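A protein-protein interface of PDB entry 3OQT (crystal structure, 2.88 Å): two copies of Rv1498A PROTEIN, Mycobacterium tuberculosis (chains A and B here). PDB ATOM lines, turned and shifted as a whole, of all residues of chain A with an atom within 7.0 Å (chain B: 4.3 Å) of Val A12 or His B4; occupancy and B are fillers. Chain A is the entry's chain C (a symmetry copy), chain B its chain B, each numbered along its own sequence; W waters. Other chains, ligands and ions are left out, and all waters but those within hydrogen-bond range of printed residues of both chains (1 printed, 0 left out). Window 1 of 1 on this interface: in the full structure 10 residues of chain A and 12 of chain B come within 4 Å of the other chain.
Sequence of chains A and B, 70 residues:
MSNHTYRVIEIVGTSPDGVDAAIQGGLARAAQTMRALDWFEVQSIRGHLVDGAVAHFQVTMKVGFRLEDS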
ATOM      1  N   GLU A  10     -11.914   1.323  -6.031  1.00  0.00           N
ATOM      2  CA  GLU A  10     -12.574   1.364  -4.736  1.00  0.00           C
ATOM      3  C   GLU A  10     -13.053  -0.015  -4.279  1.00  0.00           C
ATOM      4  O   GLU A  10     -13.945  -0.614  -4.888  1.00  0.00           O
ATOM      5  CB  GLU A  10     -13.731   2.364  -4.767  1.00  0.00           C
ATOM      6  CG  GLU A  10     -14.290   2.720  -3.398  1.00  0.00           C
ATOM      7  CD  GLU A  10     -15.191   3.936  -3.438  1.00  0.00           C
ATOM      8  OE1 GLU A  10     -14.687   5.050  -3.702  1.00  0.00           O
ATOM      9  OE2 GLU A  10     -16.407   3.782  -3.201  1.00  0.00           O
ATOM     10  N   ILE A  11     -12.448  -0.504  -3.203  1.00  0.00           N
ATOM     11  CA  ILE A  11     -12.836  -1.767  -2.590  1.00  0.00           C
ATOM     12  C   ILE A  11     -13.476  -1.532  -1.225  1.00  0.00           C
ATOM     13  O   ILE A  11     -13.175  -0.544  -0.552  1.00  0.00           O
ATOM     14  CB  ILE A  11     -11.630  -2.709  -2.410  1.00  0.00           C
ATOM     15  CG1 ILE A  11     -10.564  -2.044  -1.535  1.00  0.00           C
ATOM     16  CG2 ILE A  11     -11.065  -3.113  -3.770  1.00  0.00           C
ATOM     17  CD1 ILE A  11      -9.540  -2.981  -0.983  1.00  0.00           C
ATOM     18  N   VAL A  12     -14.364  -2.439  -0.827  1.00  0.00           N
ATOM     19  CA  VAL A  12     -14.962  -2.397   0.502  1.00  0.00           C
ATOM     20  C   VAL A  12     -14.425  -3.565   1.323  1.00  0.00           C
ATOM     21  O   VAL A  12     -14.631  -4.728   0.976  1.00  0.00           O
ATOM     22  CB  VAL A  12     -16.510  -2.428   0.447  1.00  0.00           C
ATOM     23  CG1 VAL A  12     -17.103  -2.418   1.844  1.00  0.00           C
ATOM     24  CG2 VAL A  12     -17.042  -1.256  -0.356  1.00  0.00           C
ATOM     25  N   GLY A  13     -13.713  -3.243   2.398  1.00  0.00           N
ATOM     26  CA  GLY A  13     -13.159  -4.255   3.290  1.00  0.00           C
ATOM     27  C   GLY A  13     -14.079  -4.533   4.462  1.00  0.00           C
ATOM     28  O   GLY A  13     -14.667  -3.610   5.032  1.00  0.00           O
ATOM     29  N   THR A  14     -14.203  -5.806   4.829  1.00  0.00           N
ATOM     30  CA  THR A  14     -15.122  -6.206   5.894  1.00  0.00           C
ATOM     31  C   THR A  14     -14.472  -7.124   6.924  1.00  0.00           C
ATOM     32  O   THR A  14     -13.647  -7.976   6.580  1.00  0.00           O
ATOM     33  CB  THR A  14     -16.388  -6.890   5.334  1.00  0.00           C
ATOM     34  OG1 THR A  14     -16.011  -7.976   4.481  1.00  0.00           O
ATOM     35  CG2 THR A  14     -17.240  -5.897   4.549  1.00  0.00           C
ATOM     36  N   SER A  15     -14.862  -6.937   8.183  1.00  0.00           N
ATOM     37  CA  SER A  15     -14.389  -7.762   9.291  1.00  0.00           C
ATOM     38  C   SER A  15     -15.197  -7.507  10.556  1.00  0.00           C
ATOM     39  O   SER A  15     -15.606  -6.379  10.812  1.00  0.00           O
ATOM     40  CB  SER A  15     -12.915  -7.491   9.581  1.00  0.00           C
ATOM     41  OG  SER A  15     -12.547  -8.008  10.848  1.00  0.00           O
ATOM     42  N   ALA A  22     -10.896  -5.007   8.981  1.00  0.00           N
ATOM     43  CA  ALA A  22     -11.660  -4.794   7.757  1.00  0.00           C
ATOM     44  C   ALA A  22     -10.776  -4.255   6.638  1.00  0.00           C
ATOM     45  O   ALA A  22     -10.798  -4.783   5.526  1.00  0.00           O
ATOM     46  CB  ALA A  22     -12.845  -3.874   8.015  1.00  0.00           C
ATOM     47  N   GLY A  25      -8.069  -6.892   5.611  1.00  0.00           N
ATOM     48  CA  GLY A  25      -8.745  -7.922   4.828  1.00  0.00           C
ATOM     49  C   GLY A  25      -9.116  -7.452   3.432  1.00  0.00           C
ATOM     50  O   GLY A  25      -8.944  -8.186   2.459  1.00  0.00           O
ATOM     51  N   GLY A  26      -9.629  -6.227   3.341  1.00  0.00           N
ATOM     52  CA  GLY A  26      -9.997  -5.627   2.064  1.00  0.00           C
ATOM     53  C   GLY A  26      -8.804  -5.484   1.145  1.00  0.00           C
ATOM     54  O   GLY A  26      -8.870  -5.841  -0.032  1.00  0.00           O
ATOM     55  N   LEU A  27      -7.708  -4.965   1.690  1.00  0.00           N
ATOM     56  CA  LEU A  27      -6.466  -4.814   0.940  1.00  0.00           C
ATOM     57  C   LEU A  27      -5.885  -6.160   0.523  1.00  0.00           C
ATOM     58  O   LEU A  27      -5.161  -6.245  -0.470  1.00  0.00           O
ATOM     59  CB  LEU A  27      -5.437  -4.027   1.756  1.00  0.00           C
ATOM     60  CG  LEU A  27      -5.726  -2.540   1.964  1.00  0.00           C
ATOM     61  CD1 LEU A  27      -4.674  -1.926   2.860  1.00  0.00           C
ATOM     62  CD2 LEU A  27      -5.790  -1.805   0.637  1.00  0.00           C
ATOM     63  N   ARG A  29      -7.492  -9.011  -0.582  1.00  0.00           N
ATOM     64  CA  ARG A  29      -8.073  -9.471  -1.839  1.00  0.00           C
ATOM     65  C   ARG A  29      -7.668  -8.592  -3.014  1.00  0.00           C
ATOM     66  O   ARG A  29      -7.365  -9.099  -4.097  1.00  0.00           O
ATOM     67  CB  ARG A  29      -9.588  -9.533  -1.720  1.00  0.00           C
ATOM     68  CG  ARG A  29     -10.036 -10.307  -0.512  1.00  0.00           C
ATOM     69  CD  ARG A  29     -11.238 -11.134  -0.839  1.00  0.00           C
ATOM     70  NE  ARG A  29     -11.376 -12.243   0.091  1.00  0.00           N
ATOM     71  CZ  ARG A  29     -12.281 -13.204  -0.031  1.00  0.00           C
ATOM     72  NH1 ARG A  29     -13.134 -13.195  -1.051  1.00  0.00           N
ATOM     73  NH2 ARG A  29     -12.331 -14.174   0.867  1.00  0.00           N
ATOM     74  N   HIS A  56     -20.525  -6.800  11.087  1.00  0.00           N
ATOM     75  CA  HIS A  56     -19.380  -6.663  10.190  1.00  0.00           C
ATOM     76  C   HIS A  56     -19.026  -5.198   9.959  1.00  0.00           C
ATOM     77  O   HIS A  56     -19.866  -4.418   9.513  1.00  0.00           O
ATOM     78  CB  HIS A  56     -19.660  -7.337   8.838  1.00  0.00           C
ATOM     79  CG  HIS A  56     -20.786  -8.337   8.867  1.00  0.00           C
ATOM     80  ND1 HIS A  56     -20.662  -9.586   9.438  1.00  0.00           N
ATOM     81  CD2 HIS A  56     -22.051  -8.268   8.390  1.00  0.00           C
ATOM     82  CE1 HIS A  56     -21.805 -10.240   9.317  1.00  0.00           C
ATOM     83  NE2 HIS A  56     -22.662  -9.463   8.681  1.00  0.00           N
ATOM     84  N   PHE A  57     -17.785  -4.829  10.272  1.00  0.00           N
ATOM     85  CA  PHE A  57     -17.259  -3.507   9.932  1.00  0.00           C
ATOM     86  C   PHE A  57     -17.076  -3.419   8.424  1.00  0.00           C
ATOM     87  O   PHE A  57     -16.607  -4.369   7.798  1.00  0.00           O
ATOM     88  CB  PHE A  57     -15.912  -3.258  10.617  1.00  0.00           C
ATOM     89  CG  PHE A  57     -16.011  -3.022  12.096  1.00  0.00           C
ATOM     90  CD1 PHE A  57     -16.170  -4.087  12.978  1.00  0.00           C
ATOM     91  CD2 PHE A  57     -15.928  -1.734  12.611  1.00  0.00           C
ATOM     92  CE1 PHE A  57     -16.254  -3.870  14.350  1.00  0.00           C
ATOM     93  CE2 PHE A  57     -16.013  -1.506  13.984  1.00  0.00           C
ATOM     94  CZ  PHE A  57     -16.177  -2.577  14.853  1.00  0.00           C
ATOM     95  N   GLN A  58     -17.457  -2.285   7.846  1.00  0.00           N
ATOM     96  CA  GLN A  58     -17.336  -2.069   6.408  1.00  0.00           C
ATOM     97  C   GLN A  58     -16.510  -0.822   6.128  1.00  0.00           C
ATOM     98  O   GLN A  58     -17.019   0.297   6.206  1.00  0.00           O
ATOM     99  CB  GLN A  58     -18.719  -1.916   5.768  1.00  0.00           C
ATOM    100  CG  GLN A  58     -19.613  -3.141   5.866  1.00  0.00           C
ATOM    101  CD  GLN A  58     -21.084  -2.799   5.697  1.00  0.00           C
ATOM    102  OE1 GLN A  58     -21.440  -1.815   5.046  1.00  0.00           O
ATOM    103  NE2 GLN A  58     -21.969  -3.600   6.277  1.00  0.00           N
ATOM    104  N   VAL A  59     -15.234  -1.014   5.809  1.00  0.00           N
ATOM    105  CA  VAL A  59     -14.360   0.113   5.510  1.00  0.00           C
ATOM    106  C   VAL A  59     -14.110   0.204   4.007  1.00  0.00           C
ATOM    107  O   VAL A  59     -13.299  -0.543   3.452  1.00  0.00           O
ATOM    108  CB  VAL A  59     -13.023   0.042   6.292  1.00  0.00           C
ATOM    109  CG1 VAL A  59     -12.250   1.340   6.142  1.00  0.00           C
ATOM    110  CG2 VAL A  59     -13.279  -0.242   7.764  1.00  0.00           C
ATOM    111  N   THR A  60     -14.831   1.111   3.354  1.00  0.00           N
ATOM    112  CA  THR A  60     -14.629   1.379   1.933  1.00  0.00           C
ATOM    113  C   THR A  60     -13.308   2.118   1.727  1.00  0.00           C
ATOM    114  O   THR A  60     -12.983   3.048   2.466  1.00  0.00           O
ATOM    115  CB  THR A  60     -15.803   2.179   1.324  1.00  0.00           C
ATOM    116  OG1 THR A  60     -15.540   2.452  -0.056  1.00  0.00           O
ATOM    117  CG2 THR A  60     -16.002   3.487   2.043  1.00  0.00           C
ATOM    118  N   MET A  61     -12.542   1.692   0.728  1.00  0.00           N
ATOM    119  CA  MET A  61     -11.200   2.224   0.513  1.00  0.00           C
ATOM    120  C   MET A  61     -10.919   2.580  -0.939  1.00  0.00           C
ATOM    121  O   MET A  61     -11.528   2.028  -1.852  1.00  0.00           O
ATOM    122  CB  MET A  61     -10.150   1.220   0.981  1.00  0.00           C
ATOM    123  CG  MET A  61     -10.012   1.100   2.481  1.00  0.00           C
ATOM    124  SD  MET A  61      -8.688  -0.037   2.923  1.00  0.00           S
ATOM    125  CE  MET A  61      -9.393  -1.593   2.394  1.00  0.00           C
ATOM    126  N   MET B   1     -19.755 -11.851   7.695  1.00  0.00           N
ATOM    127  CA  MET B   1     -18.751 -11.135   6.856  1.00  0.00           C
ATOM    128  C   MET B   1     -17.442 -10.863   7.599  1.00  0.00           C
ATOM    129  O   MET B   1     -17.374  -9.999   8.478  1.00  0.00           O
ATOM    130  CB  MET B   1     -19.334  -9.834   6.293  1.00  0.00           C
ATOM    131  CG  MET B   1     -20.334 -10.025   5.165  1.00  0.00           C
ATOM    132  SD  MET B   1     -21.057  -8.473   4.601  1.00  0.00           S
ATOM    133  CE  MET B   1     -22.751  -8.652   5.164  1.00  0.00           C
ATOM    134  N   SER B   2     -16.413 -11.622   7.234  1.00  0.00           N
ATOM    135  CA  SER B   2     -15.072 -11.457   7.776  1.00  0.00           C
ATOM    136  C   SER B   2     -14.091 -11.442   6.619  1.00  0.00           C
ATOM    137  O   SER B   2     -12.991 -10.900   6.723  1.00  0.00           O
ATOM    138  CB  SER B   2     -14.739 -12.608   8.723  1.00  0.00           C
ATOM    139  OG  SER B   2     -14.816 -13.855   8.052  1.00  0.00           O
ATOM    140  N   ASN B   3     -14.512 -12.052   5.516  1.00  0.00           N
ATOM    141  CA  ASN B   3     -13.711 -12.145   4.305  1.00  0.00           C
ATOM    142  C   ASN B   3     -14.563 -11.916   3.058  1.00  0.00           C
ATOM    143  O   ASN B   3     -14.448 -12.638   2.066  1.00  0.00           O
ATOM    144  CB  ASN B   3     -12.984 -13.496   4.238  1.00  0.00           C
ATOM    145  CG  ASN B   3     -13.920 -14.688   4.414  1.00  0.00           C
ATOM    146  OD1 ASN B   3     -13.464 -15.814   4.576  1.00  0.00           O
ATOM    147  ND2 ASN B   3     -15.226 -14.446   4.391  1.00  0.00           N
ATOM    148  N   HIS B   4     -15.427 -10.907   3.133  1.00  0.00           N
ATOM    149  CA  HIS B   4     -16.300 -10.542   2.024  1.00  0.00           C
ATOM    150  C   HIS B   4     -15.893  -9.177   1.484  1.00  0.00           C
ATOM    151  O   HIS B   4     -16.162  -8.149   2.103  1.00  0.00           O
ATOM    152  CB  HIS B   4     -17.762 -10.523   2.479  1.00  0.00           C
ATOM    153  CG  HIS B   4     -18.262 -11.848   2.960  1.00  0.00           C
ATOM    154  ND1 HIS B   4     -17.799 -12.448   4.112  1.00  0.00           N
ATOM    155  CD2 HIS B   4     -19.182 -12.695   2.440  1.00  0.00           C
ATOM    156  CE1 HIS B   4     -18.411 -13.606   4.280  1.00  0.00           C
ATOM    157  NE2 HIS B   4     -19.255 -13.780   3.280  1.00  0.00           N
ATOM    158  N   THR B   5     -15.229  -9.177   0.335  1.00  0.00           N
ATOM    159  CA  THR B   5     -14.759  -7.937  -0.272  1.00  0.00           C
ATOM    160  C   THR B   5     -15.672  -7.526  -1.419  1.00  0.00           C
ATOM    161  O   THR B   5     -16.302  -8.368  -2.061  1.00  0.00           O
ATOM    162  CB  THR B   5     -13.300  -8.064  -0.762  1.00  0.00           C
ATOM    163  OG1 THR B   5     -12.479  -8.524   0.316  1.00  0.00           O
ATOM    164  CG2 THR B   5     -12.760  -6.727  -1.239  1.00  0.00           C
ATOM    165  N   TYR B   6     -15.739  -6.222  -1.659  1.00  0.00           N
ATOM    166  CA  TYR B   6     -16.567  -5.672  -2.716  1.00  0.00           C
ATOM    167  C   TYR B   6     -15.741  -4.794  -3.639  1.00  0.00           C
ATOM    168  O   TYR B   6     -14.659  -4.334  -3.274  1.00  0.00           O
ATOM    169  CB  TYR B   6     -17.733  -4.881  -2.120  1.00  0.00           C
ATOM    170  CG  TYR B   6     -18.583  -5.712  -1.190  1.00  0.00           C
ATOM    171  CD1 TYR B   6     -18.218  -5.888   0.146  1.00  0.00           C
ATOM    172  CD2 TYR B   6     -19.734  -6.353  -1.652  1.00  0.00           C
ATOM    173  CE1 TYR B   6     -18.978  -6.675   1.000  1.00  0.00           C
ATOM    174  CE2 TYR B   6     -20.506  -7.142  -0.803  1.00  0.00           C
ATOM    175  CZ  TYR B   6     -20.120  -7.299   0.522  1.00  0.00           C
ATOM    176  OH  TYR B   6     -20.875  -8.080   1.368  1.00  0.00           O
ATOM    177  N   VAL B   8     -16.219  -1.363  -6.123  1.00  0.00           N
ATOM    178  CA  VAL B   8     -17.135  -0.253  -6.352  1.00  0.00           C
ATOM    179  C   VAL B   8     -16.854   0.411  -7.691  1.00  0.00           C
ATOM    180  O   VAL B   8     -15.828   1.066  -7.882  1.00  0.00           O
ATOM    181  CB  VAL B   8     -17.106   0.782  -5.213  1.00  0.00           C
ATOM    182  CG1 VAL B   8     -18.278   1.737  -5.348  1.00  0.00           C
ATOM    183  CG2 VAL B   8     -17.146   0.095  -3.854  1.00  0.00           C
ATOM    184  N   TRP B  39     -25.626  -2.932  -4.752  1.00  0.00           N
ATOM    185  CA  TRP B  39     -26.173  -1.619  -4.430  1.00  0.00           C
ATOM    186  C   TRP B  39     -25.651  -0.550  -5.384  1.00  0.00           C
ATOM    187  O   TRP B  39     -24.665  -0.759  -6.093  1.00  0.00           O
ATOM    188  CB  TRP B  39     -25.838  -1.233  -2.983  1.00  0.00           C
ATOM    189  CG  TRP B  39     -24.518  -0.548  -2.852  1.00  0.00           C
ATOM    190  CD1 TRP B  39     -24.263   0.785  -3.035  1.00  0.00           C
ATOM    191  CD2 TRP B  39     -23.265  -1.156  -2.539  1.00  0.00           C
ATOM    192  NE1 TRP B  39     -22.927   1.041  -2.859  1.00  0.00           N
ATOM    193  CE2 TRP B  39     -22.290  -0.131  -2.551  1.00  0.00           C
ATOM    194  CE3 TRP B  39     -22.867  -2.466  -2.249  1.00  0.00           C
ATOM    195  CZ2 TRP B  39     -20.939  -0.376  -2.280  1.00  0.00           C
ATOM    196  CZ3 TRP B  39     -21.524  -2.709  -1.980  1.00  0.00           C
ATOM    197  CH2 TRP B  39     -20.577  -1.667  -1.996  1.00  0.00           C
HETATM  198  O   HOH W   1     -12.557  -8.139   3.581  1.00  0.00           O
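Water W1 bridges the backbone NH (N) of Thr A14 (3.1 Å) and the side-chain hydroxyl (OG1) of Thr B5 (3.3 Å).
The backbone NH (N) of Met B1 sits at hydrogen-bond distance from a ring nitrogen (ND1) of His A56 (3.0 Å).
The backbone carbonyl oxygen of Asn B3 is in hydrogen-bond range of the guanidinium group of Arg A29 (2.9 Å).
The side-chain hydroxyl (OG1) of Thr A14 lies close to the backbone NH (N) of His B4 (3.3 Å).
The backbone NH (N) of Val A12 lies within hydrogen-bond range of the backbone carbonyl oxygen (O) of Tyr B6 (3.1 Å).
The backbone carbonyl oxygen (O) of Glu A10 lies within hydrogen-bond range of the backbone NH (N) of Val B8 (2.7 Å).
The backbone carbonyl oxygen (O) of Thr A14 lies close to the backbone carbonyl oxygen (O) of Ser B2, 3.0 Å away.
Ile A11 touches Tyr B6 (CA to O, 3.2 Å).
O of His B4 touches O of Val A12, 3.9 Å away.
Val A12 touches Thr B5 (O to CA, 3.4 Å).
Val B8 touches Val A12.
Val A12 touches Trp B39.
CA of Ser A15 touches O of Met B1, at 3.8 Å.
CD of Arg A29 touches OG1 of Thr B5, 3.1 Å away.
OH of Tyr B6 sits at hydrogen-bond distance from SD of Met B1, 3.3 Å away.
The side-chain amide nitrogen of Asn B3 lies within hydrogen-bond range of a ring nitrogen (ND1) of His B4 (3.3 Å).
O of Ile A11 sits at hydrogen-bond distance from N of Met A61 (2.7 Å).
O of Ser A15 lies within hydrogen-bond range of N of Phe A57, at 2.7 Å.
No position is printed for both chains.
Printed residues of chain B within 4 Å of Ile A11: Tyr B6.
Of chain B, only His B4 (3.9 Å), Thr B5 (3.4 Å), Tyr B6 (3.1 Å), Val B8 (3.8 Å) and Trp B39 (3.9 Å) come within 4 Å of Val A12.
Of the printed residues of chain B, Thr A14 touches Ser B2 and His B4.
Printed residues of chain B within 4 Å of Ser A15: Met B1 (3.8 Å).
Of the printed residues of chain A, His B4 touches Val A12 and Thr A14.
Printed residues of chain A within 4 Å of Thr B5: Val A12 and Arg A29.
The nearest printed residue of chain B that does not touch Val A12 is Asn B3 (7.5 Å).
The nearest residue of chain A that does not touch His B4 is Gly A13 (4.8 Å).
The nearest printed residue of chain B that does not touch Arg A29 is His B4 (5.0 Å).
Of the 8 printed residues of chain B, 8 touch a printed residue of chain A.
Hydrophobic or aromatic side chains of chain A that line the printed part of chain B: Ile A11, Val A12 and His A56.
Among the printed residues, no Asp or Glu carboxylate lies within 4 Å of a Lys or Arg side-chain nitrogen of the other chain.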
